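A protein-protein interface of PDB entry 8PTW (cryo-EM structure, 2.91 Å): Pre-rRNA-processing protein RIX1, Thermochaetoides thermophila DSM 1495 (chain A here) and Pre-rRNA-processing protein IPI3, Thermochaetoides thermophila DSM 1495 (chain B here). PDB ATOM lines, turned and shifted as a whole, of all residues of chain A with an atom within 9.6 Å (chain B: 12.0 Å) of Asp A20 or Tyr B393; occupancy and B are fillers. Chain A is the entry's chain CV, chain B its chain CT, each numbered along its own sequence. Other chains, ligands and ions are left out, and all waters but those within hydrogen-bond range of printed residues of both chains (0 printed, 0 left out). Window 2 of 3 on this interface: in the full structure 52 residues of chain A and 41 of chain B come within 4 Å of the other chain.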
ATOM      1  N   LEU A  14      -6.800 -13.570  26.249  1.00  0.00           N
ATOM      2  CA  LEU A  14      -7.822 -14.598  26.095  1.00  0.00           C
ATOM      3  C   LEU A  14      -9.123 -14.010  25.566  1.00  0.00           C
ATOM      4  O   LEU A  14      -9.860 -14.677  24.831  1.00  0.00           O
ATOM      5  CB  LEU A  14      -8.056 -15.318  27.421  1.00  0.00           C
ATOM      6  CG  LEU A  14      -7.053 -16.416  27.767  1.00  0.00           C
ATOM      7  CD1 LEU A  14      -7.490 -17.147  29.017  1.00  0.00           C
ATOM      8  CD2 LEU A  14      -6.894 -17.386  26.610  1.00  0.00           C
ATOM      9  N   SER A  16      -9.343 -11.218  23.577  1.00  0.00           N
ATOM     10  CA  SER A  16      -9.219 -10.606  22.256  1.00  0.00           C
ATOM     11  C   SER A  16      -8.957 -11.637  21.161  1.00  0.00           C
ATOM     12  O   SER A  16      -9.430 -11.474  20.029  1.00  0.00           O
ATOM     13  CB  SER A  16      -8.111  -9.555  22.271  1.00  0.00           C
ATOM     14  OG  SER A  16      -6.882 -10.114  22.698  1.00  0.00           O
ATOM     15  N   THR A  17      -8.206 -12.689  21.466  1.00  0.00           N
ATOM     16  CA  THR A  17      -7.710 -13.592  20.425  1.00  0.00           C
ATOM     17  C   THR A  17      -8.835 -14.454  19.859  1.00  0.00           C
ATOM     18  O   THR A  17      -9.689 -14.926  20.618  1.00  0.00           O
ATOM     19  CB  THR A  17      -6.605 -14.489  20.984  1.00  0.00           C
ATOM     20  OG1 THR A  17      -5.741 -13.715  21.825  1.00  0.00           O
ATOM     21  CG2 THR A  17      -5.783 -15.096  19.867  1.00  0.00           C
ATOM     22  N   PRO A  18      -8.882 -14.666  18.542  1.00  0.00           N
ATOM     23  CA  PRO A  18      -9.766 -15.701  17.993  1.00  0.00           C
ATOM     24  C   PRO A  18      -9.319 -17.084  18.438  1.00  0.00           C
ATOM     25  O   PRO A  18      -8.149 -17.309  18.756  1.00  0.00           O
ATOM     26  CB  PRO A  18      -9.621 -15.525  16.478  1.00  0.00           C
ATOM     27  CG  PRO A  18      -9.170 -14.114  16.307  1.00  0.00           C
ATOM     28  CD  PRO A  18      -8.282 -13.841  17.481  1.00  0.00           C
ATOM     29  N   VAL A  19     -10.274 -18.017  18.463  1.00  0.00           N
ATOM     30  CA  VAL A  19     -10.027 -19.322  19.074  1.00  0.00           C
ATOM     31  C   VAL A  19      -9.075 -20.162  18.225  1.00  0.00           C
ATOM     32  O   VAL A  19      -8.317 -20.983  18.755  1.00  0.00           O
ATOM     33  CB  VAL A  19     -11.358 -20.051  19.345  1.00  0.00           C
ATOM     34  CG1 VAL A  19     -12.188 -19.263  20.343  1.00  0.00           C
ATOM     35  CG2 VAL A  19     -12.149 -20.250  18.064  1.00  0.00           C
ATOM     36  N   ASP A  20      -9.084 -19.967  16.902  1.00  0.00           N
ATOM     37  CA  ASP A  20      -8.271 -20.814  16.032  1.00  0.00           C
ATOM     38  C   ASP A  20      -6.791 -20.453  16.094  1.00  0.00           C
ATOM     39  O   ASP A  20      -5.936 -21.305  15.827  1.00  0.00           O
ATOM     40  CB  ASP A  20      -8.776 -20.737  14.593  1.00  0.00           C
ATOM     41  CG  ASP A  20     -10.090 -21.467  14.400  1.00  0.00           C
ATOM     42  OD1 ASP A  20     -10.786 -21.717  15.406  1.00  0.00           O
ATOM     43  OD2 ASP A  20     -10.424 -21.798  13.243  1.00  0.00           O
ATOM     44  N   SER A  21      -6.466 -19.206  16.429  1.00  0.00           N
ATOM     45  CA  SER A  21      -5.072 -18.803  16.545  1.00  0.00           C
ATOM     46  C   SER A  21      -4.508 -19.000  17.946  1.00  0.00           C
ATOM     47  O   SER A  21      -3.312 -18.770  18.149  1.00  0.00           O
ATOM     48  CB  SER A  21      -4.915 -17.340  16.125  1.00  0.00           C
ATOM     49  OG  SER A  21      -5.761 -16.499  16.884  1.00  0.00           O
ATOM     50  N   LEU A  22      -5.340 -19.410  18.904  1.00  0.00           N
ATOM     51  CA  LEU A  22      -4.869 -19.650  20.268  1.00  0.00           C
ATOM     52  C   LEU A  22      -3.771 -20.709  20.412  1.00  0.00           C
ATOM     53  O   LEU A  22      -2.900 -20.516  21.278  1.00  0.00           O
ATOM     54  CB  LEU A  22      -6.063 -19.987  21.172  1.00  0.00           C
ATOM     55  CG  LEU A  22      -6.924 -18.813  21.634  1.00  0.00           C
ATOM     56  CD1 LEU A  22      -8.187 -19.315  22.308  1.00  0.00           C
ATOM     57  CD2 LEU A  22      -6.140 -17.912  22.568  1.00  0.00           C
ATOM     58  N   PRO A  23      -3.765 -21.846  19.679  1.00  0.00           N
ATOM     59  CA  PRO A  23      -2.617 -22.766  19.809  1.00  0.00           C
ATOM     60  C   PRO A  23      -1.271 -22.151  19.460  1.00  0.00           C
ATOM     61  O   PRO A  23      -0.249 -22.562  20.022  1.00  0.00           O
ATOM     62  CB  PRO A  23      -2.977 -23.907  18.852  1.00  0.00           C
ATOM     63  CG  PRO A  23      -4.428 -23.939  18.868  1.00  0.00           C
ATOM     64  CD  PRO A  23      -4.871 -22.512  18.959  1.00  0.00           C
ATOM     65  N   ARG A  24      -1.239 -21.178  18.549  1.00  0.00           N
ATOM     66  CA  ARG A  24       0.016 -20.501  18.251  1.00  0.00           C
ATOM     67  C   ARG A  24       0.432 -19.566  19.380  1.00  0.00           C
ATOM     68  O   ARG A  24       1.630 -19.371  19.610  1.00  0.00           O
ATOM     69  CB  ARG A  24      -0.103 -19.741  16.932  1.00  0.00           C
ATOM     70  CG  ARG A  24      -0.251 -20.657  15.733  1.00  0.00           C
ATOM     71  CD  ARG A  24      -0.022 -19.923  14.430  1.00  0.00           C
ATOM     72  NE  ARG A  24       0.034 -20.844  13.302  1.00  0.00           N
ATOM     73  CZ  ARG A  24      -1.011 -21.189  12.564  1.00  0.00           C
ATOM     74  NH1 ARG A  24      -2.218 -20.701  12.804  1.00  0.00           N
ATOM     75  NH2 ARG A  24      -0.843 -22.044  11.560  1.00  0.00           N
ATOM     76  N   LEU A  25      -0.534 -18.988  20.097  1.00  0.00           N
ATOM     77  CA  LEU A  25      -0.236 -18.147  21.251  1.00  0.00           C
ATOM     78  C   LEU A  25      -0.102 -18.930  22.548  1.00  0.00           C
ATOM     79  O   LEU A  25       0.122 -18.313  23.594  1.00  0.00           O
ATOM     80  CB  LEU A  25      -1.311 -17.067  21.438  1.00  0.00           C
ATOM     81  CG  LEU A  25      -1.340 -15.806  20.565  1.00  0.00           C
ATOM     82  CD1 LEU A  25      -1.770 -16.069  19.131  1.00  0.00           C
ATOM     83  CD2 LEU A  25      -2.244 -14.764  21.210  1.00  0.00           C
ATOM     84  N   CYS A  26      -0.256 -20.253  22.508  1.00  0.00           N
ATOM     85  CA  CYS A  26      -0.100 -21.073  23.711  1.00  0.00           C
ATOM     86  C   CYS A  26       1.225 -20.928  24.463  1.00  0.00           C
ATOM     87  O   CYS A  26       1.175 -20.952  25.703  1.00  0.00           O
ATOM     88  CB  CYS A  26      -0.346 -22.554  23.382  1.00  0.00           C
ATOM     89  SG  CYS A  26      -2.083 -23.021  23.341  1.00  0.00           S
ATOM     90  N   PRO A  27       2.414 -20.825  23.836  1.00  0.00           N
ATOM     91  CA  PRO A  27       3.630 -20.660  24.662  1.00  0.00           C
ATOM     92  C   PRO A  27       3.645 -19.409  25.532  1.00  0.00           C
ATOM     93  O   PRO A  27       4.003 -19.493  26.715  1.00  0.00           O
ATOM     94  CB  PRO A  27       4.754 -20.631  23.619  1.00  0.00           C
ATOM     95  CG  PRO A  27       4.238 -21.428  22.506  1.00  0.00           C
ATOM     96  CD  PRO A  27       2.781 -21.105  22.432  1.00  0.00           C
ATOM     97  N   LEU A  69     -13.591 -22.557  27.211  1.00  0.00           N
ATOM     98  CA  LEU A  69     -12.742 -23.080  26.143  1.00  0.00           C
ATOM     99  C   LEU A  69     -12.789 -24.601  26.098  1.00  0.00           C
ATOM    100  O   LEU A  69     -12.833 -25.202  25.018  1.00  0.00           O
ATOM    101  CB  LEU A  69     -11.302 -22.606  26.330  1.00  0.00           C
ATOM    102  CG  LEU A  69     -10.910 -21.222  25.819  1.00  0.00           C
ATOM    103  CD1 LEU A  69      -9.431 -20.981  26.075  1.00  0.00           C
ATOM    104  CD2 LEU A  69     -11.232 -21.088  24.342  1.00  0.00           C
ATOM    105  N   LYS A  73     -17.076 -26.484  21.597  1.00  0.00           N
ATOM    106  CA  LYS A  73     -16.661 -27.328  20.476  1.00  0.00           C
ATOM    107  C   LYS A  73     -15.729 -26.513  19.578  1.00  0.00           C
ATOM    108  O   LYS A  73     -16.144 -25.763  18.693  1.00  0.00           O
ATOM    109  CB  LYS A  73     -17.880 -27.863  19.730  1.00  0.00           C
ATOM    110  CG  LYS A  73     -17.599 -28.916  18.639  1.00  0.00           C
ATOM    111  CD  LYS A  73     -17.384 -28.342  17.241  1.00  0.00           C
ATOM    112  CE  LYS A  73     -17.188 -29.444  16.214  1.00  0.00           C
ATOM    113  NZ  LYS A  73     -16.942 -28.892  14.854  1.00  0.00           N
ATOM    114  N   SER A  74     -14.435 -26.643  19.862  1.00  0.00           N
ATOM    115  CA  SER A  74     -13.375 -26.085  19.032  1.00  0.00           C
ATOM    116  C   SER A  74     -12.112 -26.875  19.340  1.00  0.00           C
ATOM    117  O   SER A  74     -11.631 -26.834  20.492  1.00  0.00           O
ATOM    118  CB  SER A  74     -13.171 -24.592  19.297  1.00  0.00           C
ATOM    119  OG  SER A  74     -11.933 -24.147  18.771  1.00  0.00           O
ATOM    120  N   PRO A  75     -11.565 -27.631  18.379  1.00  0.00           N
ATOM    121  CA  PRO A  75     -10.326 -28.386  18.651  1.00  0.00           C
ATOM    122  C   PRO A  75      -9.156 -27.508  19.055  1.00  0.00           C
ATOM    123  O   PRO A  75      -8.357 -27.899  19.917  1.00  0.00           O
ATOM    124  CB  PRO A  75     -10.065 -29.106  17.322  1.00  0.00           C
ATOM    125  CG  PRO A  75     -11.403 -29.200  16.675  1.00  0.00           C
ATOM    126  CD  PRO A  75     -12.122 -27.942  17.053  1.00  0.00           C
ATOM    127  N   ALA A  76      -9.046 -26.318  18.460  1.00  0.00           N
ATOM    128  CA  ALA A  76      -8.044 -25.353  18.897  1.00  0.00           C
ATOM    129  C   ALA A  76      -8.324 -24.877  20.316  1.00  0.00           C
ATOM    130  O   ALA A  76      -7.402 -24.753  21.134  1.00  0.00           O
ATOM    131  CB  ALA A  76      -8.007 -24.174  17.929  1.00  0.00           C
ATOM    132  N   GLY A  77      -9.597 -24.613  20.625  1.00  0.00           N
ATOM    133  CA  GLY A  77      -9.961 -24.223  21.976  1.00  0.00           C
ATOM    134  C   GLY A  77      -9.723 -25.325  22.988  1.00  0.00           C
ATOM    135  O   GLY A  77      -9.277 -25.064  24.105  1.00  0.00           O
ATOM    136  N   ARG A  78     -10.011 -26.573  22.607  1.00  0.00           N
ATOM    137  CA  ARG A  78      -9.739 -27.699  23.496  1.00  0.00           C
ATOM    138  C   ARG A  78      -8.244 -27.871  23.734  1.00  0.00           C
ATOM    139  O   ARG A  78      -7.821 -28.143  24.860  1.00  0.00           O
ATOM    140  CB  ARG A  78     -10.346 -28.984  22.930  1.00  0.00           C
ATOM    141  CG  ARG A  78     -11.868 -29.001  22.922  1.00  0.00           C
ATOM    142  CD  ARG A  78     -12.411 -30.396  22.669  1.00  0.00           C
ATOM    143  NE  ARG A  78     -12.227 -30.829  21.291  1.00  0.00           N
ATOM    144  CZ  ARG A  78     -13.143 -30.705  20.341  1.00  0.00           C
ATOM    145  NH1 ARG A  78     -14.319 -30.155  20.585  1.00  0.00           N
ATOM    146  NH2 ARG A  78     -12.872 -31.144  19.116  1.00  0.00           N
ATOM    147  N   PHE A  79      -7.430 -27.703  22.686  1.00  0.00           N
ATOM    148  CA  PHE A  79      -5.976 -27.781  22.829  1.00  0.00           C
ATOM    149  C   PHE A  79      -5.453 -26.695  23.766  1.00  0.00           C
ATOM    150  O   PHE A  79      -4.640 -26.969  24.670  1.00  0.00           O
ATOM    151  CB  PHE A  79      -5.341 -27.674  21.439  1.00  0.00           C
ATOM    152  CG  PHE A  79      -3.835 -27.688  21.432  1.00  0.00           C
ATOM    153  CD1 PHE A  79      -3.112 -26.504  21.416  1.00  0.00           C
ATOM    154  CD2 PHE A  79      -3.146 -28.886  21.396  1.00  0.00           C
ATOM    155  CE1 PHE A  79      -1.733 -26.519  21.398  1.00  0.00           C
ATOM    156  CE2 PHE A  79      -1.765 -28.905  21.372  1.00  0.00           C
ATOM    157  CZ  PHE A  79      -1.060 -27.722  21.374  1.00  0.00           C
ATOM    158  N   THR A  80      -5.928 -25.460  23.575  1.00  0.00           N
ATOM    159  CA  THR A  80      -5.522 -24.350  24.431  1.00  0.00           C
ATOM    160  C   THR A  80      -5.960 -24.574  25.872  1.00  0.00           C
ATOM    161  O   THR A  80      -5.208 -24.275  26.809  1.00  0.00           O
ATOM    162  CB  THR A  80      -6.103 -23.044  23.895  1.00  0.00           C
ATOM    163  OG1 THR A  80      -5.956 -23.011  22.472  1.00  0.00           O
ATOM    164  CG2 THR A  80      -5.383 -21.852  24.501  1.00  0.00           C
ATOM    165  N   PRO A 116      -7.184 -33.958  16.995  1.00  0.00           N
ATOM    166  CA  PRO A 116      -5.787 -34.258  16.661  1.00  0.00           C
ATOM    167  C   PRO A 116      -5.094 -35.038  17.770  1.00  0.00           C
ATOM    168  O   PRO A 116      -5.358 -34.839  18.957  1.00  0.00           O
ATOM    169  CB  PRO A 116      -5.167 -32.872  16.472  1.00  0.00           C
ATOM    170  CG  PRO A 116      -6.284 -32.058  15.955  1.00  0.00           C
ATOM    171  CD  PRO A 116      -7.537 -32.575  16.613  1.00  0.00           C
ATOM    172  N   LEU A 117      -4.203 -35.943  17.358  1.00  0.00           N
ATOM    173  CA  LEU A 117      -3.648 -36.925  18.283  1.00  0.00           C
ATOM    174  C   LEU A 117      -2.654 -36.295  19.248  1.00  0.00           C
ATOM    175  O   LEU A 117      -2.393 -36.844  20.325  1.00  0.00           O
ATOM    176  CB  LEU A 117      -2.993 -38.057  17.497  1.00  0.00           C
ATOM    177  CG  LEU A 117      -3.977 -39.111  16.993  1.00  0.00           C
ATOM    178  CD1 LEU A 117      -3.254 -40.155  16.181  1.00  0.00           C
ATOM    179  CD2 LEU A 117      -4.714 -39.751  18.155  1.00  0.00           C
ATOM    180  N   SER A 118      -2.082 -35.148  18.881  1.00  0.00           N
ATOM    181  CA  SER A 118      -1.205 -34.449  19.813  1.00  0.00           C
ATOM    182  C   SER A 118      -2.001 -33.850  20.965  1.00  0.00           C
ATOM    183  O   SER A 118      -1.533 -33.827  22.111  1.00  0.00           O
ATOM    184  CB  SER A 118      -0.415 -33.368  19.085  1.00  0.00           C
ATOM    185  OG  SER A 118       0.632 -32.894  19.906  1.00  0.00           O
ATOM    186  N   SER A 119      -3.216 -33.371  20.679  1.00  0.00           N
ATOM    187  CA  SER A 119      -4.109 -32.917  21.739  1.00  0.00           C
ATOM    188  C   SER A 119      -4.500 -34.068  22.658  1.00  0.00           C
ATOM    189  O   SER A 119      -4.588 -33.892  23.877  1.00  0.00           O
ATOM    190  CB  SER A 119      -5.352 -32.267  21.132  1.00  0.00           C
ATOM    191  OG  SER A 119      -6.295 -31.929  22.133  1.00  0.00           O
ATOM    192  N   ALA B 384       8.923 -29.377  22.895  1.00  0.00           N
ATOM    193  CA  ALA B 384       7.850 -30.362  22.840  1.00  0.00           C
ATOM    194  C   ALA B 384       6.511 -29.700  22.547  1.00  0.00           C
ATOM    195  O   ALA B 384       5.694 -30.242  21.792  1.00  0.00           O
ATOM    196  CB  ALA B 384       7.792 -31.141  24.151  1.00  0.00           C
ATOM    197  N   LEU B 385       6.276 -28.516  23.118  1.00  0.00           N
ATOM    198  CA  LEU B 385       5.060 -27.771  22.811  1.00  0.00           C
ATOM    199  C   LEU B 385       5.037 -27.319  21.356  1.00  0.00           C
ATOM    200  O   LEU B 385       3.984 -27.340  20.711  1.00  0.00           O
ATOM    201  CB  LEU B 385       4.929 -26.570  23.743  1.00  0.00           C
ATOM    202  CG  LEU B 385       3.613 -25.800  23.661  1.00  0.00           C
ATOM    203  CD1 LEU B 385       2.439 -26.684  24.046  1.00  0.00           C
ATOM    204  CD2 LEU B 385       3.680 -24.569  24.538  1.00  0.00           C
ATOM    205  N   GLU B 386       6.189 -26.897  20.823  1.00  0.00           N
ATOM    206  CA  GLU B 386       6.261 -26.503  19.419  1.00  0.00           C
ATOM    207  C   GLU B 386       5.969 -27.679  18.497  1.00  0.00           C
ATOM    208  O   GLU B 386       5.234 -27.538  17.512  1.00  0.00           O
ATOM    209  CB  GLU B 386       7.634 -25.911  19.107  1.00  0.00           C
ATOM    210  CG  GLU B 386       7.790 -24.454  19.499  1.00  0.00           C
ATOM    211  CD  GLU B 386       9.179 -23.923  19.211  1.00  0.00           C
ATOM    212  OE1 GLU B 386      10.103 -24.742  19.031  1.00  0.00           O
ATOM    213  OE2 GLU B 386       9.348 -22.686  19.163  1.00  0.00           O
ATOM    214  N   SER B 387       6.524 -28.853  18.812  1.00  0.00           N
ATOM    215  CA  SER B 387       6.218 -30.048  18.032  1.00  0.00           C
ATOM    216  C   SER B 387       4.748 -30.425  18.163  1.00  0.00           C
ATOM    217  O   SER B 387       4.140 -30.919  17.207  1.00  0.00           O
ATOM    218  CB  SER B 387       7.111 -31.207  18.470  1.00  0.00           C
ATOM    219  OG  SER B 387       6.943 -31.486  19.847  1.00  0.00           O
ATOM    220  N   ALA B 388       4.156 -30.180  19.336  1.00  0.00           N
ATOM    221  CA  ALA B 388       2.730 -30.430  19.523  1.00  0.00           C
ATOM    222  C   ALA B 388       1.877 -29.510  18.656  1.00  0.00           C
ATOM    223  O   ALA B 388       0.868 -29.943  18.089  1.00  0.00           O
ATOM    224  CB  ALA B 388       2.362 -30.270  20.996  1.00  0.00           C
ATOM    225  N   ILE B 389       2.257 -28.234  18.553  1.00  0.00           N
ATOM    226  CA  ILE B 389       1.499 -27.297  17.721  1.00  0.00           C
ATOM    227  C   ILE B 389       1.661 -27.637  16.242  1.00  0.00           C
ATOM    228  O   ILE B 389       0.709 -27.530  15.459  1.00  0.00           O
ATOM    229  CB  ILE B 389       1.912 -25.844  18.025  1.00  0.00           C
ATOM    230  CG1 ILE B 389       1.692 -25.519  19.499  1.00  0.00           C
ATOM    231  CG2 ILE B 389       1.105 -24.867  17.190  1.00  0.00           C
ATOM    232  CD1 ILE B 389       2.541 -24.373  19.999  1.00  0.00           C
ATOM    233  N   VAL B 390       2.865 -28.054  15.836  1.00  0.00           N
ATOM    234  CA  VAL B 390       3.076 -28.474  14.449  1.00  0.00           C
ATOM    235  C   VAL B 390       2.257 -29.721  14.133  1.00  0.00           C
ATOM    236  O   VAL B 390       1.649 -29.828  13.060  1.00  0.00           O
ATOM    237  CB  VAL B 390       4.577 -28.684  14.169  1.00  0.00           C
ATOM    238  CG1 VAL B 390       4.794 -29.225  12.769  1.00  0.00           C
ATOM    239  CG2 VAL B 390       5.322 -27.371  14.308  1.00  0.00           C
ATOM    240  N   ALA B 391       2.203 -30.671  15.070  1.00  0.00           N
ATOM    241  CA  ALA B 391       1.393 -31.868  14.867  1.00  0.00           C
ATOM    242  C   ALA B 391      -0.095 -31.545  14.901  1.00  0.00           C
ATOM    243  O   ALA B 391      -0.909 -32.269  14.313  1.00  0.00           O
ATOM    244  CB  ALA B 391       1.738 -32.918  15.922  1.00  0.00           C
ATOM    245  N   PHE B 392      -0.474 -30.469  15.593  1.00  0.00           N
ATOM    246  CA  PHE B 392      -1.881 -30.094  15.673  1.00  0.00           C
ATOM    247  C   PHE B 392      -2.380 -29.523  14.352  1.00  0.00           C
ATOM    248  O   PHE B 392      -3.512 -29.796  13.937  1.00  0.00           O
ATOM    249  CB  PHE B 392      -2.089 -29.094  16.813  1.00  0.00           C
ATOM    250  CG  PHE B 392      -3.411 -28.382  16.767  1.00  0.00           C
ATOM    251  CD1 PHE B 392      -4.566 -29.019  17.182  1.00  0.00           C
ATOM    252  CD2 PHE B 392      -3.496 -27.071  16.326  1.00  0.00           C
ATOM    253  CE1 PHE B 392      -5.779 -28.371  17.143  1.00  0.00           C
ATOM    254  CE2 PHE B 392      -4.708 -26.420  16.281  1.00  0.00           C
ATOM    255  CZ  PHE B 392      -5.848 -27.070  16.690  1.00  0.00           C
ATOM    256  N   TYR B 393      -1.554 -28.728  13.680  1.00  0.00           N
ATOM    257  CA  TYR B 393      -1.961 -28.075  12.438  1.00  0.00           C
ATOM    258  C   TYR B 393      -1.604 -28.918  11.218  1.00  0.00           C
ATOM    259  O   TYR B 393      -2.181 -29.979  10.990  1.00  0.00           O
ATOM    260  CB  TYR B 393      -1.313 -26.694  12.327  1.00  0.00           C
ATOM    261  CG  TYR B 393      -2.046 -25.610  13.082  1.00  0.00           C
ATOM    262  CD1 TYR B 393      -1.450 -24.962  14.156  1.00  0.00           C
ATOM    263  CD2 TYR B 393      -3.333 -25.236  12.724  1.00  0.00           C
ATOM    264  CE1 TYR B 393      -2.115 -23.970  14.851  1.00  0.00           C
ATOM    265  CE2 TYR B 393      -4.006 -24.246  13.411  1.00  0.00           C
ATOM    266  CZ  TYR B 393      -3.393 -23.617  14.473  1.00  0.00           C
ATOM    267  OH  TYR B 393      -4.062 -22.631  15.159  1.00  0.00           O
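Of the 10 printed residues of chain B, 6 touch a printed residue of chain A. Hydrophobic or aromatic side chains of chain B within 4 Å of the printed part of chain A: Leu B385, Ala B388, Ile B389, Ala B391, Phe B392 and Tyr B393. Hydrophobic or aromatic side chains of chain A that line the printed part of chain B: Pro A23, Pro A27, Ala A76, Phe A79 and Pro A116. Among the printed residues, no Asp or Glu carboxylate lies within 4 Å of a Lys or Arg side-chain nitrogen of the other chain.
The backbone carbonyl oxygen (O) of Ala B388 lies close to the side-chain hydroxyl (OG) of Ser A118 (3.5 Å). The backbone carbonyl oxygen of Asp A20 lies close to the side-chain hydroxyl of Tyr B393, 2.4 Å away.
Pro A23 touches Ile B389 (O to CD1, 3.3 Å). Phe B392 touches Pro A23. OH of Tyr B393 touches CD of Pro A23, 3.9 Å away. Arg A24 touches Tyr B393 (NH1 to CZ, 3.6 Å). Pro A27 touches Leu B385. CE1 of Phe B392 touches O of Pro A75 (3.8 Å). CA of Ala A76 touches CZ of Phe B392, 3.6 Å away. CG1 of Ile B389 touches CZ of Phe A79 (3.99 Å). Pro A116 touches Phe B392. Ser A118 touches Ala B391.
Of chain B, only Tyr B393 (2.4 Å) comes within 4 Å of Asp A20. Of chain A, only Asp A20, Pro A23 and Arg A24 come within 4 Å of Tyr B393. No residue of chain B comes within 4 Å of Pro A18. No residue of chain B comes within 4 Å of Val A19. Of chain B, only Ile B389 (3.3 Å), Phe B392 (3.6 Å) and Tyr B393 (3.9 Å) come within 4 Å of Pro A23. Printed residues of chain B within 4 Å of Ala A76: Phe B392. Of the printed residues of chain B, Pro A116 touches Phe B392. Of the printed residues of chain A, Ala B388 touches Ser A118 (3.3 Å). Of the printed residues of chain A, Ala B391 touches Ser A118 (3.9 Å). Thr A80 touches none of the printed residues of chain B. Gly A77 touches none of the printed residues of chain B. The nearest residue of chain B that does not touch Asp A20 is Phe B392 (5.3 Å). The nearest printed residue of chain A that does not touch Leu B385 is Cys A26 (4.4 Å).
The backbone carbonyl oxygen (O) of Ala A76 sits at hydrogen-bond distance from the side-chain hydroxyl (OG1) of Thr A80 (2.6 Å).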
